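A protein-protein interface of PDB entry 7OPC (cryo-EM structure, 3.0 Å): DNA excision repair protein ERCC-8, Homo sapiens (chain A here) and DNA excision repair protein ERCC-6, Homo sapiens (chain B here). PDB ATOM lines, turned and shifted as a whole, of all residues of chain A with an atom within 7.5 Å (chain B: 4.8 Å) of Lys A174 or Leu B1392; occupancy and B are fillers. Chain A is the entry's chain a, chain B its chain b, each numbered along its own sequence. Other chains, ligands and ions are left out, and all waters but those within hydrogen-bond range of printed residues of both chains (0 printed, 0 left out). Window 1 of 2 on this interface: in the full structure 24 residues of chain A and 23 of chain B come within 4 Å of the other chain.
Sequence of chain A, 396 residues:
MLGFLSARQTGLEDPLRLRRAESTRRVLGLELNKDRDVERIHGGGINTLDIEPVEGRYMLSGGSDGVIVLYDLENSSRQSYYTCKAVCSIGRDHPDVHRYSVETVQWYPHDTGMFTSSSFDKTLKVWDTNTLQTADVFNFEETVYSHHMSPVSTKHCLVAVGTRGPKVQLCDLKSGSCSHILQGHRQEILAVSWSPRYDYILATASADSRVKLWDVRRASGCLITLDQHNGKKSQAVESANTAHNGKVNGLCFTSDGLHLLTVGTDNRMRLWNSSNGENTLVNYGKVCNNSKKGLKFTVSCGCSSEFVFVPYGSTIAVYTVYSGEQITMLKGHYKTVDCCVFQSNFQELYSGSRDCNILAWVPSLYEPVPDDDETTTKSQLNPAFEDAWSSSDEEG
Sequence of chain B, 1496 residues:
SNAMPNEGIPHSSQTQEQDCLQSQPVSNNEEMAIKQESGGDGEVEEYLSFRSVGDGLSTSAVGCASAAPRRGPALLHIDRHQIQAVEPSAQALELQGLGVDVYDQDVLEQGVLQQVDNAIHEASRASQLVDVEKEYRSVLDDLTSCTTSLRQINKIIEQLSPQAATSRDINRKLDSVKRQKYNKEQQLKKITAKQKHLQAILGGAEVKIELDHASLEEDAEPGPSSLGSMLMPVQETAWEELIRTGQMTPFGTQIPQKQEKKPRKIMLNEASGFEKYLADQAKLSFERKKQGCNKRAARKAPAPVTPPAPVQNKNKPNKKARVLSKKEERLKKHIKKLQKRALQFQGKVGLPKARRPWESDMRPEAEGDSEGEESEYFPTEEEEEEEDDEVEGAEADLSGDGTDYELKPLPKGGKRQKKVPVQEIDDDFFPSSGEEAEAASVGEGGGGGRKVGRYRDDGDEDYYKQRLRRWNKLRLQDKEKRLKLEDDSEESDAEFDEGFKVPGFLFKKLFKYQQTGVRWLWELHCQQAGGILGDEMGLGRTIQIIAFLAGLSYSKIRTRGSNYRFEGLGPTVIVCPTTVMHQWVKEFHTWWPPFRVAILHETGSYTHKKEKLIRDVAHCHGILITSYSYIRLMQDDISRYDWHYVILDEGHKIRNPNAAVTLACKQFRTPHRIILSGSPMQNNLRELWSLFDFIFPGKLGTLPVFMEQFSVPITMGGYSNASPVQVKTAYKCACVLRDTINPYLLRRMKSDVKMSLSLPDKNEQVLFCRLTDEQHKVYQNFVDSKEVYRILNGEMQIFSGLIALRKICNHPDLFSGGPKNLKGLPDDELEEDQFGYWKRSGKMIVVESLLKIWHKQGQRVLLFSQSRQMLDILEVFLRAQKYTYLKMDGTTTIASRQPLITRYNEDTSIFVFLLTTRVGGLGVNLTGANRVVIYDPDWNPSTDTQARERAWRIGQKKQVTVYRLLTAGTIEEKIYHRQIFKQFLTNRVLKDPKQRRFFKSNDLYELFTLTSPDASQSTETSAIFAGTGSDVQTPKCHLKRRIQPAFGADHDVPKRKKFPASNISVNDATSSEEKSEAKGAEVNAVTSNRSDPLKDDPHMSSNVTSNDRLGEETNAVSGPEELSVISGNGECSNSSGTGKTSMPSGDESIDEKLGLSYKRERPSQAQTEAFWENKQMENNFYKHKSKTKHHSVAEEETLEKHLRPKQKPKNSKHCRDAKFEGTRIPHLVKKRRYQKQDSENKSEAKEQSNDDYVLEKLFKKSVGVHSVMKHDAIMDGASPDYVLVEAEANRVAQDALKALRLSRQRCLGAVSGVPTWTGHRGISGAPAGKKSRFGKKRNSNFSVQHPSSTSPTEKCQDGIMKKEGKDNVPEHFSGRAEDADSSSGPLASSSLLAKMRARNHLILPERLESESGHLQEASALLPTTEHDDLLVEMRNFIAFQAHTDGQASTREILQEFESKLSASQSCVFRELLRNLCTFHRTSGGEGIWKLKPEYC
Tyr A108 touches Ser B1389 (CE2 to CB, 3.6 Å). OH of Tyr A108 touches CD1 of Leu B1392 (3.95 Å). CE of Met A114 touches CD1 of Leu B1392, at 3.97 Å. Val A126 touches Met B1396 (CG1 to SD, 3.9 Å). Ala A135 touches Leu B1393. Ala A135 touches Met B1396. Met B1396 touches Asp A136. Met B1396 touches Leu A173. Leu B1392 touches Lys A174. CA of Ser A175 touches NE of Arg B1399, 3.6 Å away.
The backbone NH (N) of Gly A176 sits close to the guanidinium group (NE) of Arg B1399 (3.2 Å). OH of Tyr A108 sits at hydrogen-bond distance from O of Leu B1387, at 2.6 Å. NH1 of Arg B1399 is in salt-bridge range of OD2 of Asp A136 (3.7 Å). The guanidinium group of Arg B1399 lies within hydrogen-bond range of the backbone carbonyl oxygen of Leu A173 (3.2 Å).
Of chain B, only Leu B1392 comes within 4 Å of Lys A174. Of chain A, only Tyr A108, Met A114, Cys A157 and Lys A174 come within 4 Å of Leu B1392. No residue of chain A comes within 4 Å of Ser B1391. Of the printed residues of chain B, Ala A135 touches Leu B1393 and Met B1396. Of the printed residues of chain A, Ser B1389 touches Tyr A108. Of the printed residues of chain A, Leu B1393 touches Met A114 and Ala A135. Printed residues of chain B within 4 Å of Asp A136: Met B1396 and Arg B1399. Leu A158 touches none of the printed residues of chain B. Cys A171 touches none of the printed residues of chain B. The nearest residue of chain B that does not touch Lys A174 is Arg B1399 (4.5 Å). The nearest printed residue of chain B that does not touch Cys A157 is Met B1396 (6.3 Å).
N of Tyr A108 lies close to O of Met A114 (3.0 Å). The backbone NH (N) of Val A126 lies within hydrogen-bond range of the backbone carbonyl oxygen (O) of Asp A136, 3.0 Å away. O of Cys A157 lies within hydrogen-bond range of N of Leu A173, at 3.2 Å. O of Val A126 lies within hydrogen-bond range of N of Ala A135 (2.7 Å). OD1 of Asp A172 sits close to N of Lys A174 (3.2 Å).
Hydrophobic or aromatic side chains of chain A within 4 Å of the printed part of chain B: Tyr A108, Met A114, Val A126, Ala A135 and Leu A173. Of the 10 printed residues of chain B, 6 touch a printed residue of chain A. Among the printed residues, 16 pairs touch across the chains.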
ATOM      1  N   TYR A 108     -21.196  -9.056  -5.999  1.00  0.00           N
ATOM      2  CA  TYR A 108     -20.965  -9.085  -4.594  1.00  0.00           C
ATOM      3  C   TYR A 108     -22.225  -8.550  -3.943  1.00  0.00           C
ATOM      4  O   TYR A 108     -22.624  -7.423  -4.247  1.00  0.00           O
ATOM      5  CB  TYR A 108     -19.790  -8.211  -4.262  1.00  0.00           C
ATOM      6  CG  TYR A 108     -19.548  -7.992  -2.806  1.00  0.00           C
ATOM      7  CD1 TYR A 108     -19.343  -9.050  -1.956  1.00  0.00           C
ATOM      8  CD2 TYR A 108     -19.446  -6.718  -2.298  1.00  0.00           C
ATOM      9  CE1 TYR A 108     -19.090  -8.849  -0.632  1.00  0.00           C
ATOM     10  CE2 TYR A 108     -19.196  -6.503  -0.977  1.00  0.00           C
ATOM     11  CZ  TYR A 108     -19.011  -7.571  -0.146  1.00  0.00           C
ATOM     12  OH  TYR A 108     -18.755  -7.353   1.183  1.00  0.00           O
ATOM     13  N   PRO A 109     -22.893  -9.293  -3.076  1.00  0.00           N
ATOM     14  CA  PRO A 109     -24.000  -8.689  -2.350  1.00  0.00           C
ATOM     15  C   PRO A 109     -23.443  -7.602  -1.459  1.00  0.00           C
ATOM     16  O   PRO A 109     -22.261  -7.596  -1.113  1.00  0.00           O
ATOM     17  CB  PRO A 109     -24.577  -9.854  -1.552  1.00  0.00           C
ATOM     18  CG  PRO A 109     -23.427 -10.714  -1.326  1.00  0.00           C
ATOM     19  CD  PRO A 109     -22.568 -10.619  -2.532  1.00  0.00           C
ATOM     20  N   MET A 114     -17.915  -4.657  -6.808  1.00  0.00           N
ATOM     21  CA  MET A 114     -17.116  -5.848  -7.004  1.00  0.00           C
ATOM     22  C   MET A 114     -18.031  -6.986  -7.420  1.00  0.00           C
ATOM     23  O   MET A 114     -19.131  -7.128  -6.889  1.00  0.00           O
ATOM     24  CB  MET A 114     -16.346  -6.148  -5.704  1.00  0.00           C
ATOM     25  CG  MET A 114     -15.402  -7.338  -5.725  1.00  0.00           C
ATOM     26  SD  MET A 114     -16.183  -8.926  -5.447  1.00  0.00           S
ATOM     27  CE  MET A 114     -16.497  -8.792  -3.703  1.00  0.00           C
ATOM     28  N   VAL A 126     -12.092 -12.446  -9.052  1.00  0.00           N
ATOM     29  CA  VAL A 126     -12.796 -11.352  -8.405  1.00  0.00           C
ATOM     30  C   VAL A 126     -12.467 -10.079  -9.153  1.00  0.00           C
ATOM     31  O   VAL A 126     -11.292  -9.782  -9.392  1.00  0.00           O
ATOM     32  CB  VAL A 126     -12.396 -11.229  -6.932  1.00  0.00           C
ATOM     33  CG1 VAL A 126     -13.070 -10.045  -6.326  1.00  0.00           C
ATOM     34  CG2 VAL A 126     -12.767 -12.467  -6.196  1.00  0.00           C
ATOM     35  N   ALA A 135      -9.121  -8.198  -9.056  1.00  0.00           N
ATOM     36  CA  ALA A 135      -8.481  -7.961  -7.773  1.00  0.00           C
ATOM     37  C   ALA A 135      -7.885  -9.217  -7.183  1.00  0.00           C
ATOM     38  O   ALA A 135      -6.994  -9.129  -6.336  1.00  0.00           O
ATOM     39  CB  ALA A 135      -9.479  -7.385  -6.782  1.00  0.00           C
ATOM     40  N   ASP A 136      -8.358 -10.376  -7.611  1.00  0.00           N
ATOM     41  CA  ASP A 136      -7.922 -11.627  -7.033  1.00  0.00           C
ATOM     42  C   ASP A 136      -8.235 -12.708  -8.045  1.00  0.00           C
ATOM     43  O   ASP A 136      -9.135 -12.560  -8.872  1.00  0.00           O
ATOM     44  CB  ASP A 136      -8.629 -11.886  -5.703  1.00  0.00           C
ATOM     45  CG  ASP A 136      -7.797 -12.696  -4.739  1.00  0.00           C
ATOM     46  OD1 ASP A 136      -6.709 -13.167  -5.121  1.00  0.00           O
ATOM     47  OD2 ASP A 136      -8.235 -12.857  -3.584  1.00  0.00           O
ATOM     48  N   PHE A 138      -8.500 -17.038  -7.852  1.00  0.00           N
ATOM     49  CA  PHE A 138      -8.397 -18.303  -7.155  1.00  0.00           C
ATOM     50  C   PHE A 138      -8.293 -19.339  -8.250  1.00  0.00           C
ATOM     51  O   PHE A 138      -9.097 -19.348  -9.183  1.00  0.00           O
ATOM     52  CB  PHE A 138      -9.598 -18.558  -6.265  1.00  0.00           C
ATOM     53  CG  PHE A 138      -9.738 -17.576  -5.165  1.00  0.00           C
ATOM     54  CD1 PHE A 138     -10.316 -16.350  -5.384  1.00  0.00           C
ATOM     55  CD2 PHE A 138      -9.269 -17.872  -3.919  1.00  0.00           C
ATOM     56  CE1 PHE A 138     -10.438 -15.452  -4.369  1.00  0.00           C
ATOM     57  CE2 PHE A 138      -9.387 -16.981  -2.898  1.00  0.00           C
ATOM     58  CZ  PHE A 138      -9.970 -15.766  -3.121  1.00  0.00           C
ATOM     59  N   MET A 149     -21.778 -16.532  -3.592  1.00  0.00           N
ATOM     60  CA  MET A 149     -21.530 -15.749  -2.389  1.00  0.00           C
ATOM     61  C   MET A 149     -22.818 -15.591  -1.600  1.00  0.00           C
ATOM     62  O   MET A 149     -23.899 -15.482  -2.178  1.00  0.00           O
ATOM     63  CB  MET A 149     -20.980 -14.370  -2.733  1.00  0.00           C
ATOM     64  CG  MET A 149     -19.529 -14.375  -3.061  1.00  0.00           C
ATOM     65  SD  MET A 149     -18.870 -12.778  -3.529  1.00  0.00           S
ATOM     66  CE  MET A 149     -19.657 -12.585  -5.111  1.00  0.00           C
ATOM     67  N   LYS A 155     -21.018 -10.861   7.850  1.00  0.00           N
ATOM     68  CA  LYS A 155     -19.893 -11.273   8.682  1.00  0.00           C
ATOM     69  C   LYS A 155     -18.801 -11.980   7.887  1.00  0.00           C
ATOM     70  O   LYS A 155     -17.647 -11.545   7.903  1.00  0.00           O
ATOM     71  CB  LYS A 155     -20.394 -12.191   9.807  1.00  0.00           C
ATOM     72  N   HIS A 156     -19.140 -13.062   7.188  1.00  0.00           N
ATOM     73  CA  HIS A 156     -18.171 -13.833   6.426  1.00  0.00           C
ATOM     74  C   HIS A 156     -18.308 -13.449   4.963  1.00  0.00           C
ATOM     75  O   HIS A 156     -19.352 -12.951   4.539  1.00  0.00           O
ATOM     76  CB  HIS A 156     -18.374 -15.346   6.596  1.00  0.00           C
ATOM     77  CG  HIS A 156     -19.515 -15.920   5.804  1.00  0.00           C
ATOM     78  ND1 HIS A 156     -19.442 -16.139   4.448  1.00  0.00           N
ATOM     79  CD2 HIS A 156     -20.744 -16.341   6.178  1.00  0.00           C
ATOM     80  CE1 HIS A 156     -20.573 -16.662   4.018  1.00  0.00           C
ATOM     81  NE2 HIS A 156     -21.380 -16.798   5.050  1.00  0.00           N
ATOM     82  N   CYS A 157     -17.243 -13.654   4.198  1.00  0.00           N
ATOM     83  CA  CYS A 157     -17.301 -13.317   2.785  1.00  0.00           C
ATOM     84  C   CYS A 157     -16.746 -14.489   1.989  1.00  0.00           C
ATOM     85  O   CYS A 157     -15.888 -14.333   1.118  1.00  0.00           O
ATOM     86  CB  CYS A 157     -16.546 -12.023   2.526  1.00  0.00           C
ATOM     87  SG  CYS A 157     -16.647 -11.474   0.840  1.00  0.00           S
ATOM     88  N   LEU A 158     -17.227 -15.675   2.330  1.00  0.00           N
ATOM     89  CA  LEU A 158     -16.845 -16.911   1.678  1.00  0.00           C
ATOM     90  C   LEU A 158     -17.542 -17.057   0.339  1.00  0.00           C
ATOM     91  O   LEU A 158     -18.689 -16.639   0.174  1.00  0.00           O
ATOM     92  CB  LEU A 158     -17.221 -18.086   2.566  1.00  0.00           C
ATOM     93  CG  LEU A 158     -16.473 -18.155   3.885  1.00  0.00           C
ATOM     94  CD1 LEU A 158     -17.143 -19.166   4.767  1.00  0.00           C
ATOM     95  CD2 LEU A 158     -15.024 -18.519   3.675  1.00  0.00           C
ATOM     96  N   CYS A 171     -13.801 -20.214  -0.567  1.00  0.00           N
ATOM     97  CA  CYS A 171     -12.786 -19.210  -0.830  1.00  0.00           C
ATOM     98  C   CYS A 171     -13.142 -17.970  -0.034  1.00  0.00           C
ATOM     99  O   CYS A 171     -14.179 -17.351  -0.282  1.00  0.00           O
ATOM    100  CB  CYS A 171     -12.720 -18.888  -2.317  1.00  0.00           C
ATOM    101  SG  CYS A 171     -12.637 -20.338  -3.343  1.00  0.00           S
ATOM    102  N   ASP A 172     -12.281 -17.597   0.897  1.00  0.00           N
ATOM    103  CA  ASP A 172     -12.511 -16.424   1.724  1.00  0.00           C
ATOM    104  C   ASP A 172     -11.913 -15.229   1.001  1.00  0.00           C
ATOM    105  O   ASP A 172     -10.707 -15.181   0.764  1.00  0.00           O
ATOM    106  CB  ASP A 172     -11.896 -16.608   3.104  1.00  0.00           C
ATOM    107  CG  ASP A 172     -12.517 -15.702   4.133  1.00  0.00           C
ATOM    108  OD1 ASP A 172     -12.539 -14.476   3.912  1.00  0.00           O
ATOM    109  OD2 ASP A 172     -13.013 -16.217   5.156  1.00  0.00           O
ATOM    110  N   LEU A 173     -12.763 -14.286   0.613  1.00  0.00           N
ATOM    111  CA  LEU A 173     -12.293 -13.102  -0.091  1.00  0.00           C
ATOM    112  C   LEU A 173     -11.533 -12.172   0.842  1.00  0.00           C
ATOM    113  O   LEU A 173     -10.485 -11.630   0.475  1.00  0.00           O
ATOM    114  CB  LEU A 173     -13.481 -12.407  -0.733  1.00  0.00           C
ATOM    115  CG  LEU A 173     -14.157 -13.209  -1.842  1.00  0.00           C
ATOM    116  CD1 LEU A 173     -15.386 -12.506  -2.339  1.00  0.00           C
ATOM    117  CD2 LEU A 173     -13.220 -13.424  -2.981  1.00  0.00           C
ATOM    118  N   LYS A 174     -12.049 -11.966   2.051  1.00  0.00           N
ATOM    119  CA  LYS A 174     -11.214 -11.502   3.149  1.00  0.00           C
ATOM    120  C   LYS A 174     -10.100 -12.530   3.244  1.00  0.00           C
ATOM    121  O   LYS A 174     -10.328 -13.675   2.850  1.00  0.00           O
ATOM    122  CB  LYS A 174     -12.017 -11.409   4.445  1.00  0.00           C
ATOM    123  N   SER A 175      -8.977 -12.208   3.885  1.00  0.00           N
ATOM    124  CA  SER A 175      -7.660 -12.681   3.454  1.00  0.00           C
ATOM    125  C   SER A 175      -7.675 -14.031   2.750  1.00  0.00           C
ATOM    126  O   SER A 175      -8.150 -15.027   3.300  1.00  0.00           O
ATOM    127  CB  SER A 175      -6.742 -12.785   4.663  1.00  0.00           C
ATOM    128  OG  SER A 175      -5.444 -13.214   4.285  1.00  0.00           O
ATOM    129  N   GLY A 176      -7.124 -14.062   1.540  1.00  0.00           N
ATOM    130  CA  GLY A 176      -7.462 -15.073   0.562  1.00  0.00           C
ATOM    131  C   GLY A 176      -7.065 -16.464   0.980  1.00  0.00           C
ATOM    132  O   GLY A 176      -5.894 -16.833   0.879  1.00  0.00           O
ATOM    133  N   SER A 177      -8.041 -17.264   1.392  1.00  0.00           N
ATOM    134  CA  SER A 177      -7.791 -18.583   1.963  1.00  0.00           C
ATOM    135  C   SER A 177      -8.685 -19.582   1.245  1.00  0.00           C
ATOM    136  O   SER A 177      -9.830 -19.798   1.645  1.00  0.00           O
ATOM    137  CB  SER A 177      -8.056 -18.575   3.459  1.00  0.00           C
ATOM    138  OG  SER A 177      -7.893 -19.865   4.004  1.00  0.00           O
ATOM    139  N   CYS A 178      -8.141 -20.222   0.215  1.00  0.00           N
ATOM    140  CA  CYS A 178      -8.877 -21.174  -0.603  1.00  0.00           C
ATOM    141  C   CYS A 178      -8.565 -22.612  -0.237  1.00  0.00           C
ATOM    142  O   CYS A 178      -8.604 -23.495  -1.097  1.00  0.00           O
ATOM    143  CB  CYS A 178      -8.561 -20.928  -2.070  1.00  0.00           C
ATOM    144  SG  CYS A 178      -6.807 -21.032  -2.436  1.00  0.00           S
ATOM    145  N   LEU B1387     -18.166  -5.561   4.841  1.00  0.00           N
ATOM    146  CA  LEU B1387     -17.050  -4.915   4.187  1.00  0.00           C
ATOM    147  C   LEU B1387     -17.525  -4.345   2.880  1.00  0.00           C
ATOM    148  O   LEU B1387     -18.209  -5.015   2.112  1.00  0.00           O
ATOM    149  CB  LEU B1387     -15.924  -5.900   3.936  1.00  0.00           C
ATOM    150  CG  LEU B1387     -14.972  -6.222   5.079  1.00  0.00           C
ATOM    151  CD1 LEU B1387     -14.160  -5.015   5.483  1.00  0.00           C
ATOM    152  CD2 LEU B1387     -15.715  -6.765   6.268  1.00  0.00           C
ATOM    153  N   SER B1389     -16.465  -3.660  -0.070  1.00  0.00           N
ATOM    154  CA  SER B1389     -15.966  -3.939  -1.417  1.00  0.00           C
ATOM    155  C   SER B1389     -14.924  -2.967  -1.895  1.00  0.00           C
ATOM    156  O   SER B1389     -14.641  -2.910  -3.071  1.00  0.00           O
ATOM    157  CB  SER B1389     -17.079  -3.921  -2.444  1.00  0.00           C
ATOM    158  OG  SER B1389     -17.281  -2.588  -2.820  1.00  0.00           O
ATOM    159  N   SER B1390     -14.408  -2.200  -1.078  1.00  0.00           N
ATOM    160  CA  SER B1390     -13.247  -1.415  -1.356  1.00  0.00           C
ATOM    161  C   SER B1390     -12.234  -1.681  -0.289  1.00  0.00           C
ATOM    162  O   SER B1390     -11.051  -1.730  -0.562  1.00  0.00           O
ATOM    163  CB  SER B1390     -13.598   0.014  -1.381  1.00  0.00           C
ATOM    164  OG  SER B1390     -14.645   0.214  -2.286  1.00  0.00           O
ATOM    165  N   SER B1391     -12.687  -1.879   0.928  1.00  0.00           N
ATOM    166  CA  SER B1391     -11.831  -2.517   1.886  1.00  0.00           C
ATOM    167  C   SER B1391     -11.429  -3.878   1.385  1.00  0.00           C
ATOM    168  O   SER B1391     -10.253  -4.241   1.442  1.00  0.00           O
ATOM    169  CB  SER B1391     -12.553  -2.627   3.197  1.00  0.00           C
ATOM    170  OG  SER B1391     -13.820  -3.144   2.925  1.00  0.00           O
ATOM    171  N   LEU B1392     -12.372  -4.641   0.864  1.00  0.00           N
ATOM    172  CA  LEU B1392     -11.989  -5.911   0.293  1.00  0.00           C
ATOM    173  C   LEU B1392     -11.013  -5.712  -0.819  1.00  0.00           C
ATOM    174  O   LEU B1392      -9.943  -6.299  -0.806  1.00  0.00           O
ATOM    175  CB  LEU B1392     -13.178  -6.647  -0.258  1.00  0.00           C
ATOM    176  CG  LEU B1392     -14.019  -7.424   0.726  1.00  0.00           C
ATOM    177  CD1 LEU B1392     -15.076  -8.069  -0.068  1.00  0.00           C
ATOM    178  CD2 LEU B1392     -13.307  -8.461   1.507  1.00  0.00           C
ATOM    179  N   LEU B1393     -11.343  -4.889  -1.782  1.00  0.00           N
ATOM    180  CA  LEU B1393     -10.485  -4.847  -2.938  1.00  0.00           C
ATOM    181  C   LEU B1393      -9.162  -4.247  -2.588  1.00  0.00           C
ATOM    182  O   LEU B1393      -8.150  -4.587  -3.186  1.00  0.00           O
ATOM    183  CB  LEU B1393     -11.115  -4.070  -4.049  1.00  0.00           C
ATOM    184  CG  LEU B1393     -12.324  -4.701  -4.650  1.00  0.00           C
ATOM    185  CD1 LEU B1393     -12.871  -3.736  -5.525  1.00  0.00           C
ATOM    186  CD2 LEU B1393     -11.991  -5.855  -5.447  1.00  0.00           C
ATOM    187  N   ALA B1394      -9.141  -3.328  -1.649  1.00  0.00           N
ATOM    188  CA  ALA B1394      -7.862  -2.823  -1.215  1.00  0.00           C
ATOM    189  C   ALA B1394      -7.041  -3.935  -0.612  1.00  0.00           C
ATOM    190  O   ALA B1394      -5.860  -4.079  -0.922  1.00  0.00           O
ATOM    191  CB  ALA B1394      -8.068  -1.707  -0.215  1.00  0.00           C
ATOM    192  N   LYS B1395      -7.655  -4.751   0.229  1.00  0.00           N
ATOM    193  CA  LYS B1395      -6.921  -5.835   0.840  1.00  0.00           C
ATOM    194  C   LYS B1395      -6.440  -6.812  -0.201  1.00  0.00           C
ATOM    195  O   LYS B1395      -5.315  -7.305  -0.139  1.00  0.00           O
ATOM    196  CB  LYS B1395      -7.796  -6.524   1.862  1.00  0.00           C
ATOM    197  CG  LYS B1395      -7.914  -5.721   3.092  1.00  0.00           C
ATOM    198  CD  LYS B1395      -8.771  -6.377   4.135  1.00  0.00           C
ATOM    199  CE  LYS B1395      -8.683  -5.601   5.425  1.00  0.00           C
ATOM    200  NZ  LYS B1395      -9.401  -6.190   6.555  1.00  0.00           N
ATOM    201  N   MET B1396      -7.273  -7.097  -1.172  1.00  0.00           N
ATOM    202  CA  MET B1396      -6.868  -7.991  -2.231  1.00  0.00           C
ATOM    203  C   MET B1396      -5.701  -7.418  -2.991  1.00  0.00           C
ATOM    204  O   MET B1396      -4.749  -8.126  -3.311  1.00  0.00           O
ATOM    205  CB  MET B1396      -8.019  -8.236  -3.180  1.00  0.00           C
ATOM    206  CG  MET B1396      -8.903  -9.313  -2.760  1.00  0.00           C
ATOM    207  SD  MET B1396     -10.500  -9.152  -3.486  1.00  0.00           S
ATOM    208  CE  MET B1396     -11.384 -10.186  -2.398  1.00  0.00           C
ATOM    209  N   ARG B1399      -2.508  -7.883  -0.973  1.00  0.00           N
ATOM    210  CA  ARG B1399      -1.953  -9.222  -0.972  1.00  0.00           C
ATOM    211  C   ARG B1399      -1.360  -9.575  -2.315  1.00  0.00           C
ATOM    212  O   ARG B1399      -0.300 -10.184  -2.379  1.00  0.00           O
ATOM    213  CB  ARG B1399      -3.022 -10.225  -0.630  1.00  0.00           C
ATOM    214  CG  ARG B1399      -3.168 -10.458   0.800  1.00  0.00           C
ATOM    215  CD  ARG B1399      -3.976 -11.669   1.065  1.00  0.00           C
ATOM    216  NE  ARG B1399      -5.396 -11.409   0.935  1.00  0.00           N
ATOM    217  CZ  ARG B1399      -6.092 -11.518  -0.182  1.00  0.00           C
ATOM    218  NH1 ARG B1399      -5.510 -11.887  -1.308  1.00  0.00           N
ATOM    219  NH2 ARG B1399      -7.388 -11.257  -0.163  1.00  0.00           N
